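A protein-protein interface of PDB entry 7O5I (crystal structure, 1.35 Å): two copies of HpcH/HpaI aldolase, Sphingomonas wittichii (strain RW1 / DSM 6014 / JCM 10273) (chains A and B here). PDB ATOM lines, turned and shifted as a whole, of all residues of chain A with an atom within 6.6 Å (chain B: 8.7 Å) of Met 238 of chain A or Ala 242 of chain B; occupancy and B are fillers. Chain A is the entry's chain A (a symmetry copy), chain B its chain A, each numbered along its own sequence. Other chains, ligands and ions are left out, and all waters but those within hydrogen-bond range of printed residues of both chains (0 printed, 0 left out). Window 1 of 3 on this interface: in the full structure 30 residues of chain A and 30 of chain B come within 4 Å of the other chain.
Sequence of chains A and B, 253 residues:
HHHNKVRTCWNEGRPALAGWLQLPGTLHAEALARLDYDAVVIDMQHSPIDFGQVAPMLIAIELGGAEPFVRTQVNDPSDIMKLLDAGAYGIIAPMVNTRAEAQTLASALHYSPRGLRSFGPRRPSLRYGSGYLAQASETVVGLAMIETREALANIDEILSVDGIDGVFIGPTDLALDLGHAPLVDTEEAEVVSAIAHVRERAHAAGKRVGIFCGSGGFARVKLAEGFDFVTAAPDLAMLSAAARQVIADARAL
The backbone carbonyl oxygen (O) of Trp 20 of chain A lies within hydrogen-bond range of the backbone NH (N) of Asp 235 of chain A. The backbone carbonyl oxygen of Ala 232 of chain A lies within hydrogen-bond range of the side-chain hydroxyl of Tyr 37 of chain A (2.7 Å).
Leu 35 of chain A touches Ala 243 of chain B. CD2 of Leu 35 of chain A touches NH2 of Arg 244 of chain B (3.4 Å). CD1 of Ile 247 of chain B touches CB of Leu 35 of chain A, 3.6 Å away. Tyr 37 of chain A touches Ile 247 of chain B (CE1 to CG1, 3.6 Å). O of Ala 232 of chain A touches CG1 of Val 246 of chain B, at 3.6 Å. CE of Met 238 of chain A touches CD1 of Leu 239 of chain B, 3.9 Å away. Met 238 of chain A touches Ala 243 of chain B. Met 238 of chain A touches Val 246 of chain B. Leu 239 of chain A touches Met 238 of chain B. Met 238 of chain B touches Ala 242 of chain A.
Of the printed residues of chain B, Met 238 of chain A touches Leu 239, Ala 242, Ala 243 and Val 246. Of the printed residues of chain A, Ala 242 of chain B touches Met 238. Printed residues of chain A within 4 Å of Met 238 of chain B: Leu 239, Ala 242 and Ala 243. Printed residues of chain B within 4 Å of Leu 32 of chain A: Ala 243. Of the printed residues of chain A, Arg 244 of chain B touches Leu 35 (3.4 Å). Of the printed residues of chain A, Leu 35 of chain B touches Ala 243. Printed residues of chain B within 4 Å of Leu 239 of chain A: Asp 235 and Met 238. The nearest residue of chain A that does not touch Ala 242 of chain B is Ala 242 of chain A (4.7 Å). The nearest printed residue of chain A that does not touch Arg 244 of chain B is Tyr 37 of chain A (6.1 Å).
Leu 32 of chain A touches Ala 243 of chain B, and with the chains exchanged Ala 243 of chain A touches Leu 32 of chain B. Leu 35 of chain A touches Ala 243 of chain B, and with the chains exchanged Ala 243 of chain A touches Leu 35 of chain B. Asp 235 of chain A touches Leu 239 of chain B, and with the chains exchanged Leu 239 of chain A touches Asp 235 of chain B. Met 238 of chain A touches Ala 242 of chain B, and with the chains exchanged Ala 242 of chain A touches Met 238 of chain B. 11 positions are printed for both chains. Of the 18 pairs that touch across the chains among the printed residues, 12 have their exchanged pair printed and touching as well.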
ATOM      1  N   TRP A  20      35.017  -8.748 -29.519  1.00  0.00           N
ATOM      2  CA  TRP A  20      35.557  -8.681 -30.870  1.00  0.00           C
ATOM      3  C   TRP A  20      35.390  -7.256 -31.363  1.00  0.00           C
ATOM      4  O   TRP A  20      34.261  -6.790 -31.551  1.00  0.00           O
ATOM      5  CB  TRP A  20      34.811  -9.649 -31.809  1.00  0.00           C
ATOM      6  CG  TRP A  20      35.516  -9.889 -33.102  1.00  0.00           C
ATOM      7  CD1 TRP A  20      35.425  -9.167 -34.233  1.00  0.00           C
ATOM      8  CD2 TRP A  20      36.403 -10.968 -33.393  1.00  0.00           C
ATOM      9  NE1 TRP A  20      36.259  -9.676 -35.194  1.00  0.00           N
ATOM     10  CE2 TRP A  20      36.870 -10.794 -34.706  1.00  0.00           C
ATOM     11  CE3 TRP A  20      36.841 -12.066 -32.660  1.00  0.00           C
ATOM     12  CZ2 TRP A  20      37.750 -11.697 -35.329  1.00  0.00           C
ATOM     13  CZ3 TRP A  20      37.746 -12.959 -33.264  1.00  0.00           C
ATOM     14  CH2 TRP A  20      38.198 -12.752 -34.580  1.00  0.00           C
ATOM     15  N   LEU A  32      34.270  -2.281 -22.846  1.00  0.00           N
ATOM     16  CA  LEU A  32      33.910  -3.680 -23.063  1.00  0.00           C
ATOM     17  C   LEU A  32      34.796  -4.623 -22.261  1.00  0.00           C
ATOM     18  O   LEU A  32      34.306  -5.640 -21.754  1.00  0.00           O
ATOM     19  CB  LEU A  32      33.948  -4.009 -24.556  1.00  0.00           C
ATOM     20  CG  LEU A  32      32.570  -3.809 -25.234  1.00  0.00           C
ATOM     21  CD1 LEU A  32      31.971  -2.427 -24.982  1.00  0.00           C
ATOM     22  CD2 LEU A  32      32.684  -4.136 -26.727  1.00  0.00           C
ATOM     23  N   LEU A  35      33.421  -5.377 -18.865  1.00  0.00           N
ATOM     24  CA  LEU A  35      32.296  -6.292 -18.786  1.00  0.00           C
ATOM     25  C   LEU A  35      32.824  -7.710 -18.526  1.00  0.00           C
ATOM     26  O   LEU A  35      34.034  -7.950 -18.389  1.00  0.00           O
ATOM     27  CB  LEU A  35      31.487  -6.219 -20.074  1.00  0.00           C
ATOM     28  CG  LEU A  35      30.965  -4.831 -20.456  1.00  0.00           C
ATOM     29  CD1 LEU A  35      30.214  -4.897 -21.780  1.00  0.00           C
ATOM     30  CD2 LEU A  35      30.109  -4.291 -19.333  1.00  0.00           C
ATOM     31  N   TYR A  37      33.794 -10.214 -19.983  1.00  0.00           N
ATOM     32  CA  TYR A  37      34.580 -10.838 -21.033  1.00  0.00           C
ATOM     33  C   TYR A  37      35.924 -11.229 -20.438  1.00  0.00           C
ATOM     34  O   TYR A  37      36.546 -10.430 -19.725  1.00  0.00           O
ATOM     35  CB  TYR A  37      34.867  -9.869 -22.186  1.00  0.00           C
ATOM     36  CG  TYR A  37      33.804  -9.612 -23.222  1.00  0.00           C
ATOM     37  CD1 TYR A  37      33.142 -10.651 -23.855  1.00  0.00           C
ATOM     38  CD2 TYR A  37      33.545  -8.313 -23.667  1.00  0.00           C
ATOM     39  CE1 TYR A  37      32.211 -10.393 -24.864  1.00  0.00           C
ATOM     40  CE2 TYR A  37      32.651  -8.049 -24.675  1.00  0.00           C
ATOM     41  CZ  TYR A  37      31.998  -9.088 -25.285  1.00  0.00           C
ATOM     42  OH  TYR A  37      31.153  -8.812 -26.312  1.00  0.00           O
ATOM     43  N   GLY A 214      28.145 -14.517 -33.935  1.00  0.00           N
ATOM     44  CA  GLY A 214      27.470 -13.283 -34.234  1.00  0.00           C
ATOM     45  C   GLY A 214      26.369 -12.902 -33.277  1.00  0.00           C
ATOM     46  O   GLY A 214      25.765 -11.834 -33.438  1.00  0.00           O
ATOM     47  N   ALA A 232      31.833 -13.182 -29.131  1.00  0.00           N
ATOM     48  CA  ALA A 232      30.499 -12.683 -29.457  1.00  0.00           C
ATOM     49  C   ALA A 232      30.384 -11.266 -28.908  1.00  0.00           C
ATOM     50  O   ALA A 232      30.695 -11.068 -27.724  1.00  0.00           O
ATOM     51  CB  ALA A 232      29.408 -13.539 -28.804  1.00  0.00           C
ATOM     52  N   ALA A 233      29.941 -10.267 -29.699  1.00  0.00           N
ATOM     53  CA  ALA A 233      29.838 -10.275 -31.157  1.00  0.00           C
ATOM     54  C   ALA A 233      30.577  -8.986 -31.578  1.00  0.00           C
ATOM     55  O   ALA A 233      30.911  -8.160 -30.724  1.00  0.00           O
ATOM     56  CB  ALA A 233      28.417 -10.256 -31.610  1.00  0.00           C
ATOM     57  N   PRO A 234      30.825  -8.786 -32.872  1.00  0.00           N
ATOM     58  CA  PRO A 234      31.608  -7.609 -33.280  1.00  0.00           C
ATOM     59  C   PRO A 234      30.974  -6.303 -32.808  1.00  0.00           C
ATOM     60  O   PRO A 234      29.760  -6.088 -32.947  1.00  0.00           O
ATOM     61  CB  PRO A 234      31.631  -7.709 -34.809  1.00  0.00           C
ATOM     62  CG  PRO A 234      31.518  -9.173 -35.080  1.00  0.00           C
ATOM     63  CD  PRO A 234      30.581  -9.692 -34.011  1.00  0.00           C
ATOM     64  N   ASP A 235      31.821  -5.405 -32.310  1.00  0.00           N
ATOM     65  CA  ASP A 235      31.367  -4.077 -31.883  1.00  0.00           C
ATOM     66  C   ASP A 235      30.534  -3.385 -32.945  1.00  0.00           C
ATOM     67  O   ASP A 235      29.444  -2.900 -32.645  1.00  0.00           O
ATOM     68  CB  ASP A 235      32.541  -3.223 -31.372  1.00  0.00           C
ATOM     69  CG  ASP A 235      33.689  -3.055 -32.365  1.00  0.00           C
ATOM     70  OD1 ASP A 235      33.682  -3.598 -33.493  1.00  0.00           O
ATOM     71  OD2 ASP A 235      34.640  -2.359 -31.971  1.00  0.00           O
ATOM     72  N   LEU A 236      31.029  -3.327 -34.178  1.00  0.00           N
ATOM     73  CA  LEU A 236      30.321  -2.599 -35.222  1.00  0.00           C
ATOM     74  C   LEU A 236      28.950  -3.220 -35.469  1.00  0.00           C
ATOM     75  O   LEU A 236      27.957  -2.502 -35.620  1.00  0.00           O
ATOM     76  CB  LEU A 236      31.148  -2.587 -36.507  1.00  0.00           C
ATOM     77  CG  LEU A 236      30.484  -1.980 -37.741  1.00  0.00           C
ATOM     78  CD1 LEU A 236      30.042  -0.534 -37.510  1.00  0.00           C
ATOM     79  CD2 LEU A 236      31.415  -2.096 -38.958  1.00  0.00           C
ATOM     80  N   ALA A 237      28.875  -4.560 -35.525  1.00  0.00           N
ATOM     81  CA  ALA A 237      27.586  -5.214 -35.769  1.00  0.00           C
ATOM     82  C   ALA A 237      26.612  -4.956 -34.623  1.00  0.00           C
ATOM     83  O   ALA A 237      25.430  -4.657 -34.843  1.00  0.00           O
ATOM     84  CB  ALA A 237      27.794  -6.716 -35.962  1.00  0.00           C
ATOM     85  N   MET A 238      27.084  -5.061 -33.386  1.00  0.00           N
ATOM     86  CA  MET A 238      26.195  -4.830 -32.249  1.00  0.00           C
ATOM     87  C   MET A 238      25.744  -3.370 -32.215  1.00  0.00           C
ATOM     88  O   MET A 238      24.574  -3.075 -31.944  1.00  0.00           O
ATOM     89  CB  MET A 238      26.926  -5.162 -30.952  1.00  0.00           C
ATOM     90  CG  MET A 238      27.334  -6.592 -30.776  1.00  0.00           C
ATOM     91  SD  MET A 238      27.816  -7.034 -29.083  1.00  0.00           S
ATOM     92  CE  MET A 238      29.323  -6.071 -28.853  1.00  0.00           C
ATOM     93  N   LEU A 239      26.659  -2.444 -32.497  1.00  0.00           N
ATOM     94  CA  LEU A 239      26.322  -1.023 -32.467  1.00  0.00           C
ATOM     95  C   LEU A 239      25.320  -0.675 -33.572  1.00  0.00           C
ATOM     96  O   LEU A 239      24.355   0.065 -33.342  1.00  0.00           O
ATOM     97  CB  LEU A 239      27.619  -0.209 -32.589  1.00  0.00           C
ATOM     98  CG  LEU A 239      27.448   1.306 -32.772  1.00  0.00           C
ATOM     99  CD1 LEU A 239      26.615   1.915 -31.626  1.00  0.00           C
ATOM    100  CD2 LEU A 239      28.806   1.929 -32.846  1.00  0.00           C
ATOM    101  N   SER A 240      25.577  -1.151 -34.793  1.00  0.00           N
ATOM    102  CA  SER A 240      24.649  -0.924 -35.890  1.00  0.00           C
ATOM    103  C   SER A 240      23.264  -1.417 -35.522  1.00  0.00           C
ATOM    104  O   SER A 240      22.269  -0.690 -35.648  1.00  0.00           O
ATOM    105  CB  SER A 240      25.142  -1.650 -37.134  1.00  0.00           C
ATOM    106  OG  SER A 240      26.304  -1.054 -37.637  1.00  0.00           O
ATOM    107  N   ALA A 241      23.178  -2.661 -35.066  1.00  0.00           N
ATOM    108  CA  ALA A 241      21.876  -3.242 -34.767  1.00  0.00           C
ATOM    109  C   ALA A 241      21.178  -2.450 -33.667  1.00  0.00           C
ATOM    110  O   ALA A 241      19.960  -2.212 -33.732  1.00  0.00           O
ATOM    111  CB  ALA A 241      22.016  -4.710 -34.377  1.00  0.00           C
ATOM    112  N   ALA A 242      21.939  -1.999 -32.675  1.00  0.00           N
ATOM    113  CA  ALA A 242      21.344  -1.235 -31.585  1.00  0.00           C
ATOM    114  C   ALA A 242      20.805   0.088 -32.105  1.00  0.00           C
ATOM    115  O   ALA A 242      19.697   0.506 -31.744  1.00  0.00           O
ATOM    116  CB  ALA A 242      22.372  -0.955 -30.497  1.00  0.00           C
ATOM    117  N   ALA A 243      21.568   0.759 -32.968  1.00  0.00           N
ATOM    118  CA  ALA A 243      21.133   2.046 -33.507  1.00  0.00           C
ATOM    119  C   ALA A 243      19.902   1.870 -34.382  1.00  0.00           C
ATOM    120  O   ALA A 243      18.961   2.668 -34.323  1.00  0.00           O
ATOM    121  CB  ALA A 243      22.288   2.679 -34.304  1.00  0.00           C
ATOM    122  N   LEU B  32      26.348   4.378 -39.197  1.00  0.00           N
ATOM    123  CA  LEU B  32      25.176   4.977 -38.564  1.00  0.00           C
ATOM    124  C   LEU B  32      24.551   6.056 -39.436  1.00  0.00           C
ATOM    125  O   LEU B  32      23.320   6.174 -39.476  1.00  0.00           O
ATOM    126  CB  LEU B  32      25.542   5.517 -37.181  1.00  0.00           C
ATOM    127  CG  LEU B  32      25.303   4.472 -36.063  1.00  0.00           C
ATOM    128  CD1 LEU B  32      25.982   3.132 -36.336  1.00  0.00           C
ATOM    129  CD2 LEU B  32      25.707   5.069 -34.711  1.00  0.00           C
ATOM    130  N   LEU B  35      21.928   4.723 -41.746  1.00  0.00           N
ATOM    131  CA  LEU B  35      20.640   4.378 -41.169  1.00  0.00           C
ATOM    132  C   LEU B  35      19.692   5.576 -41.314  1.00  0.00           C
ATOM    133  O   LEU B  35      20.038   6.628 -41.875  1.00  0.00           O
ATOM    134  CB  LEU B  35      20.824   3.978 -39.711  1.00  0.00           C
ATOM    135  CG  LEU B  35      21.802   2.828 -39.453  1.00  0.00           C
ATOM    136  CD1 LEU B  35      21.920   2.564 -37.957  1.00  0.00           C
ATOM    137  CD2 LEU B  35      21.351   1.606 -40.221  1.00  0.00           C
ATOM    138  N   ASP B 235      26.558   6.333 -29.124  1.00  0.00           N
ATOM    139  CA  ASP B 235      27.195   5.101 -29.601  1.00  0.00           C
ATOM    140  C   ASP B 235      27.757   4.267 -28.466  1.00  0.00           C
ATOM    141  O   ASP B 235      27.482   3.069 -28.395  1.00  0.00           O
ATOM    142  CB  ASP B 235      28.221   5.395 -30.711  1.00  0.00           C
ATOM    143  CG  ASP B 235      29.309   6.395 -30.325  1.00  0.00           C
ATOM    144  OD1 ASP B 235      29.340   6.950 -29.203  1.00  0.00           O
ATOM    145  OD2 ASP B 235      30.152   6.635 -31.206  1.00  0.00           O
ATOM    146  N   LEU B 236      28.540   4.876 -27.580  1.00  0.00           N
ATOM    147  CA  LEU B 236      29.182   4.114 -26.518  1.00  0.00           C
ATOM    148  C   LEU B 236      28.135   3.471 -25.614  1.00  0.00           C
ATOM    149  O   LEU B 236      28.271   2.306 -25.229  1.00  0.00           O
ATOM    150  CB  LEU B 236      30.111   5.018 -25.711  1.00  0.00           C
ATOM    151  CG  LEU B 236      30.758   4.403 -24.471  1.00  0.00           C
ATOM    152  CD1 LEU B 236      31.572   3.151 -24.804  1.00  0.00           C
ATOM    153  CD2 LEU B 236      31.612   5.451 -23.740  1.00  0.00           C
ATOM    154  N   ALA B 237      27.082   4.223 -25.251  1.00  0.00           N
ATOM    155  CA  ALA B 237      26.048   3.664 -24.375  1.00  0.00           C
ATOM    156  C   ALA B 237      25.312   2.514 -25.057  1.00  0.00           C
ATOM    157  O   ALA B 237      25.060   1.465 -24.447  1.00  0.00           O
ATOM    158  CB  ALA B 237      25.061   4.760 -23.971  1.00  0.00           C
ATOM    159  N   MET B 238      24.961   2.681 -26.326  1.00  0.00           N
ATOM    160  CA  MET B 238      24.249   1.614 -27.029  1.00  0.00           C
ATOM    161  C   MET B 238      25.149   0.389 -27.185  1.00  0.00           C
ATOM    162  O   MET B 238      24.700  -0.752 -27.015  1.00  0.00           O
ATOM    163  CB  MET B 238      23.822   2.105 -28.408  1.00  0.00           C
ATOM    164  CG  MET B 238      22.841   3.236 -28.428  1.00  0.00           C
ATOM    165  SD  MET B 238      22.048   3.516 -30.037  1.00  0.00           S
ATOM    166  CE  MET B 238      23.434   4.063 -31.053  1.00  0.00           C
ATOM    167  N   LEU B 239      26.425   0.607 -27.498  1.00  0.00           N
ATOM    168  CA  LEU B 239      27.351  -0.507 -27.688  1.00  0.00           C
ATOM    169  C   LEU B 239      27.581  -1.257 -26.373  1.00  0.00           C
ATOM    170  O   LEU B 239      27.594  -2.495 -26.344  1.00  0.00           O
ATOM    171  CB  LEU B 239      28.662   0.040 -28.275  1.00  0.00           C
ATOM    172  CG  LEU B 239      29.828  -0.955 -28.362  1.00  0.00           C
ATOM    173  CD1 LEU B 239      29.432  -2.205 -29.175  1.00  0.00           C
ATOM    174  CD2 LEU B 239      31.000  -0.257 -28.977  1.00  0.00           C
ATOM    175  N   SER B 240      27.829  -0.518 -25.290  1.00  0.00           N
ATOM    176  CA  SER B 240      27.999  -1.141 -23.987  1.00  0.00           C
ATOM    177  C   SER B 240      26.795  -2.000 -23.651  1.00  0.00           C
ATOM    178  O   SER B 240      26.927  -3.177 -23.291  1.00  0.00           O
ATOM    179  CB  SER B 240      28.177  -0.065 -22.925  1.00  0.00           C
ATOM    180  OG  SER B 240      29.406   0.587 -23.071  1.00  0.00           O
ATOM    181  N   ALA B 241      25.605  -1.422 -23.760  1.00  0.00           N
ATOM    182  CA  ALA B 241      24.401  -2.149 -23.378  1.00  0.00           C
ATOM    183  C   ALA B 241      24.233  -3.394 -24.242  1.00  0.00           C
ATOM    184  O   ALA B 241      23.853  -4.467 -23.743  1.00  0.00           O
ATOM    185  CB  ALA B 241      23.173  -1.249 -23.473  1.00  0.00           C
ATOM    186  N   ALA B 242      24.551  -3.281 -25.527  1.00  0.00           N
ATOM    187  CA  ALA B 242      24.415  -4.427 -26.418  1.00  0.00           C
ATOM    188  C   ALA B 242      25.389  -5.523 -26.017  1.00  0.00           C
ATOM    189  O   ALA B 242      25.030  -6.706 -25.979  1.00  0.00           O
ATOM    190  CB  ALA B 242      24.691  -4.026 -27.861  1.00  0.00           C
ATOM    191  N   ALA B 243      26.628  -5.148 -25.699  1.00  0.00           N
ATOM    192  CA  ALA B 243      27.633  -6.137 -25.314  1.00  0.00           C
ATOM    193  C   ALA B 243      27.253  -6.803 -24.001  1.00  0.00           C
ATOM    194  O   ALA B 243      27.390  -8.020 -23.842  1.00  0.00           O
ATOM    195  CB  ALA B 243      29.006  -5.451 -25.205  1.00  0.00           C
ATOM    196  N   ARG B 244      26.753  -6.026 -23.042  1.00  0.00           N
ATOM    197  CA  ARG B 244      26.354  -6.593 -21.760  1.00  0.00           C
ATOM    198  C   ARG B 244      25.257  -7.633 -21.972  1.00  0.00           C
ATOM    199  O   ARG B 244      25.259  -8.694 -21.345  1.00  0.00           O
ATOM    200  CB  ARG B 244      25.927  -5.451 -20.823  1.00  0.00           C
ATOM    201  CG  ARG B 244      25.548  -5.877 -19.442  1.00  0.00           C
ATOM    202  CD  ARG B 244      25.157  -4.632 -18.634  1.00  0.00           C
ATOM    203  NE  ARG B 244      26.290  -3.822 -18.185  1.00  0.00           N
ATOM    204  CZ  ARG B 244      27.078  -4.145 -17.167  1.00  0.00           C
ATOM    205  NH1 ARG B 244      26.914  -5.278 -16.497  1.00  0.00           N
ATOM    206  NH2 ARG B 244      28.051  -3.310 -16.806  1.00  0.00           N
ATOM    207  N   GLN B 245      24.365  -7.384 -22.905  1.00  0.00           N
ATOM    208  CA  GLN B 245      23.290  -8.323 -23.157  1.00  0.00           C
ATOM    209  C   GLN B 245      23.785  -9.551 -23.894  1.00  0.00           C
ATOM    210  O   GLN B 245      23.296 -10.651 -23.643  1.00  0.00           O
ATOM    211  CB  GLN B 245      22.148  -7.651 -23.912  1.00  0.00           C
ATOM    212  CG  GLN B 245      20.933  -8.545 -24.059  1.00  0.00           C
ATOM    213  CD  GLN B 245      20.306  -8.829 -22.700  1.00  0.00           C
ATOM    214  OE1 GLN B 245      19.929  -7.899 -21.984  1.00  0.00           O
ATOM    215  NE2 GLN B 245      20.171 -10.107 -22.346  1.00  0.00           N
ATOM    216  N   VAL B 246      24.715  -9.382 -24.824  1.00  0.00           N
ATOM    217  CA  VAL B 246      25.292 -10.540 -25.507  1.00  0.00           C
ATOM    218  C   VAL B 246      25.991 -11.443 -24.521  1.00  0.00           C
ATOM    219  O   VAL B 246      25.824 -12.668 -24.575  1.00  0.00           O
ATOM    220  CB  VAL B 246      26.230 -10.089 -26.636  1.00  0.00           C
ATOM    221  CG1 VAL B 246      27.112 -11.260 -27.099  1.00  0.00           C
ATOM    222  CG2 VAL B 246      25.426  -9.563 -27.843  1.00  0.00           C
ATOM    223  N   ILE B 247      26.742 -10.861 -23.581  1.00  0.00           N
ATOM    224  CA  ILE B 247      27.422 -11.629 -22.540  1.00  0.00           C
ATOM    225  C   ILE B 247      26.406 -12.366 -21.681  1.00  0.00           C
ATOM    226  O   ILE B 247      26.559 -13.563 -21.411  1.00  0.00           O
ATOM    227  CB  ILE B 247      28.333 -10.704 -21.709  1.00  0.00           C
ATOM    228  CG1 ILE B 247      29.463 -10.158 -22.590  1.00  0.00           C
ATOM    229  CG2 ILE B 247      28.848 -11.408 -20.478  1.00  0.00           C
ATOM    230  CD1 ILE B 247      30.258  -9.047 -21.912  1.00  0.00           C
ATOM    231  N   ALA B 248      25.331 -11.681 -21.275  1.00  0.00           N
ATOM    232  CA  ALA B 248      24.331 -12.322 -20.420  1.00  0.00           C
ATOM    233  C   ALA B 248      23.682 -13.489 -21.139  1.00  0.00           C
ATOM    234  O   ALA B 248      23.526 -14.586 -20.562  1.00  0.00           O
ATOM    235  CB  ALA B 248      23.263 -11.301 -19.998  1.00  0.00           C
ATOM    236  N   ASP B 249      23.385 -13.302 -22.423  1.00  0.00           N
ATOM    237  CA  ASP B 249      22.793 -14.362 -23.230  1.00  0.00           C
ATOM    238  C   ASP B 249      23.773 -15.521 -23.431  1.00  0.00           C
ATOM    239  O   ASP B 249      23.386 -16.700 -23.371  1.00  0.00           O
ATOM    240  CB  ASP B 249      22.372 -13.798 -24.582  1.00  0.00           C
ATOM    241  CG  ASP B 249      21.208 -12.844 -24.478  1.00  0.00           C
ATOM    242  OD1 ASP B 249      20.576 -12.783 -23.411  1.00  0.00           O
ATOM    243  OD2 ASP B 249      20.907 -12.169 -25.488  1.00  0.00           O
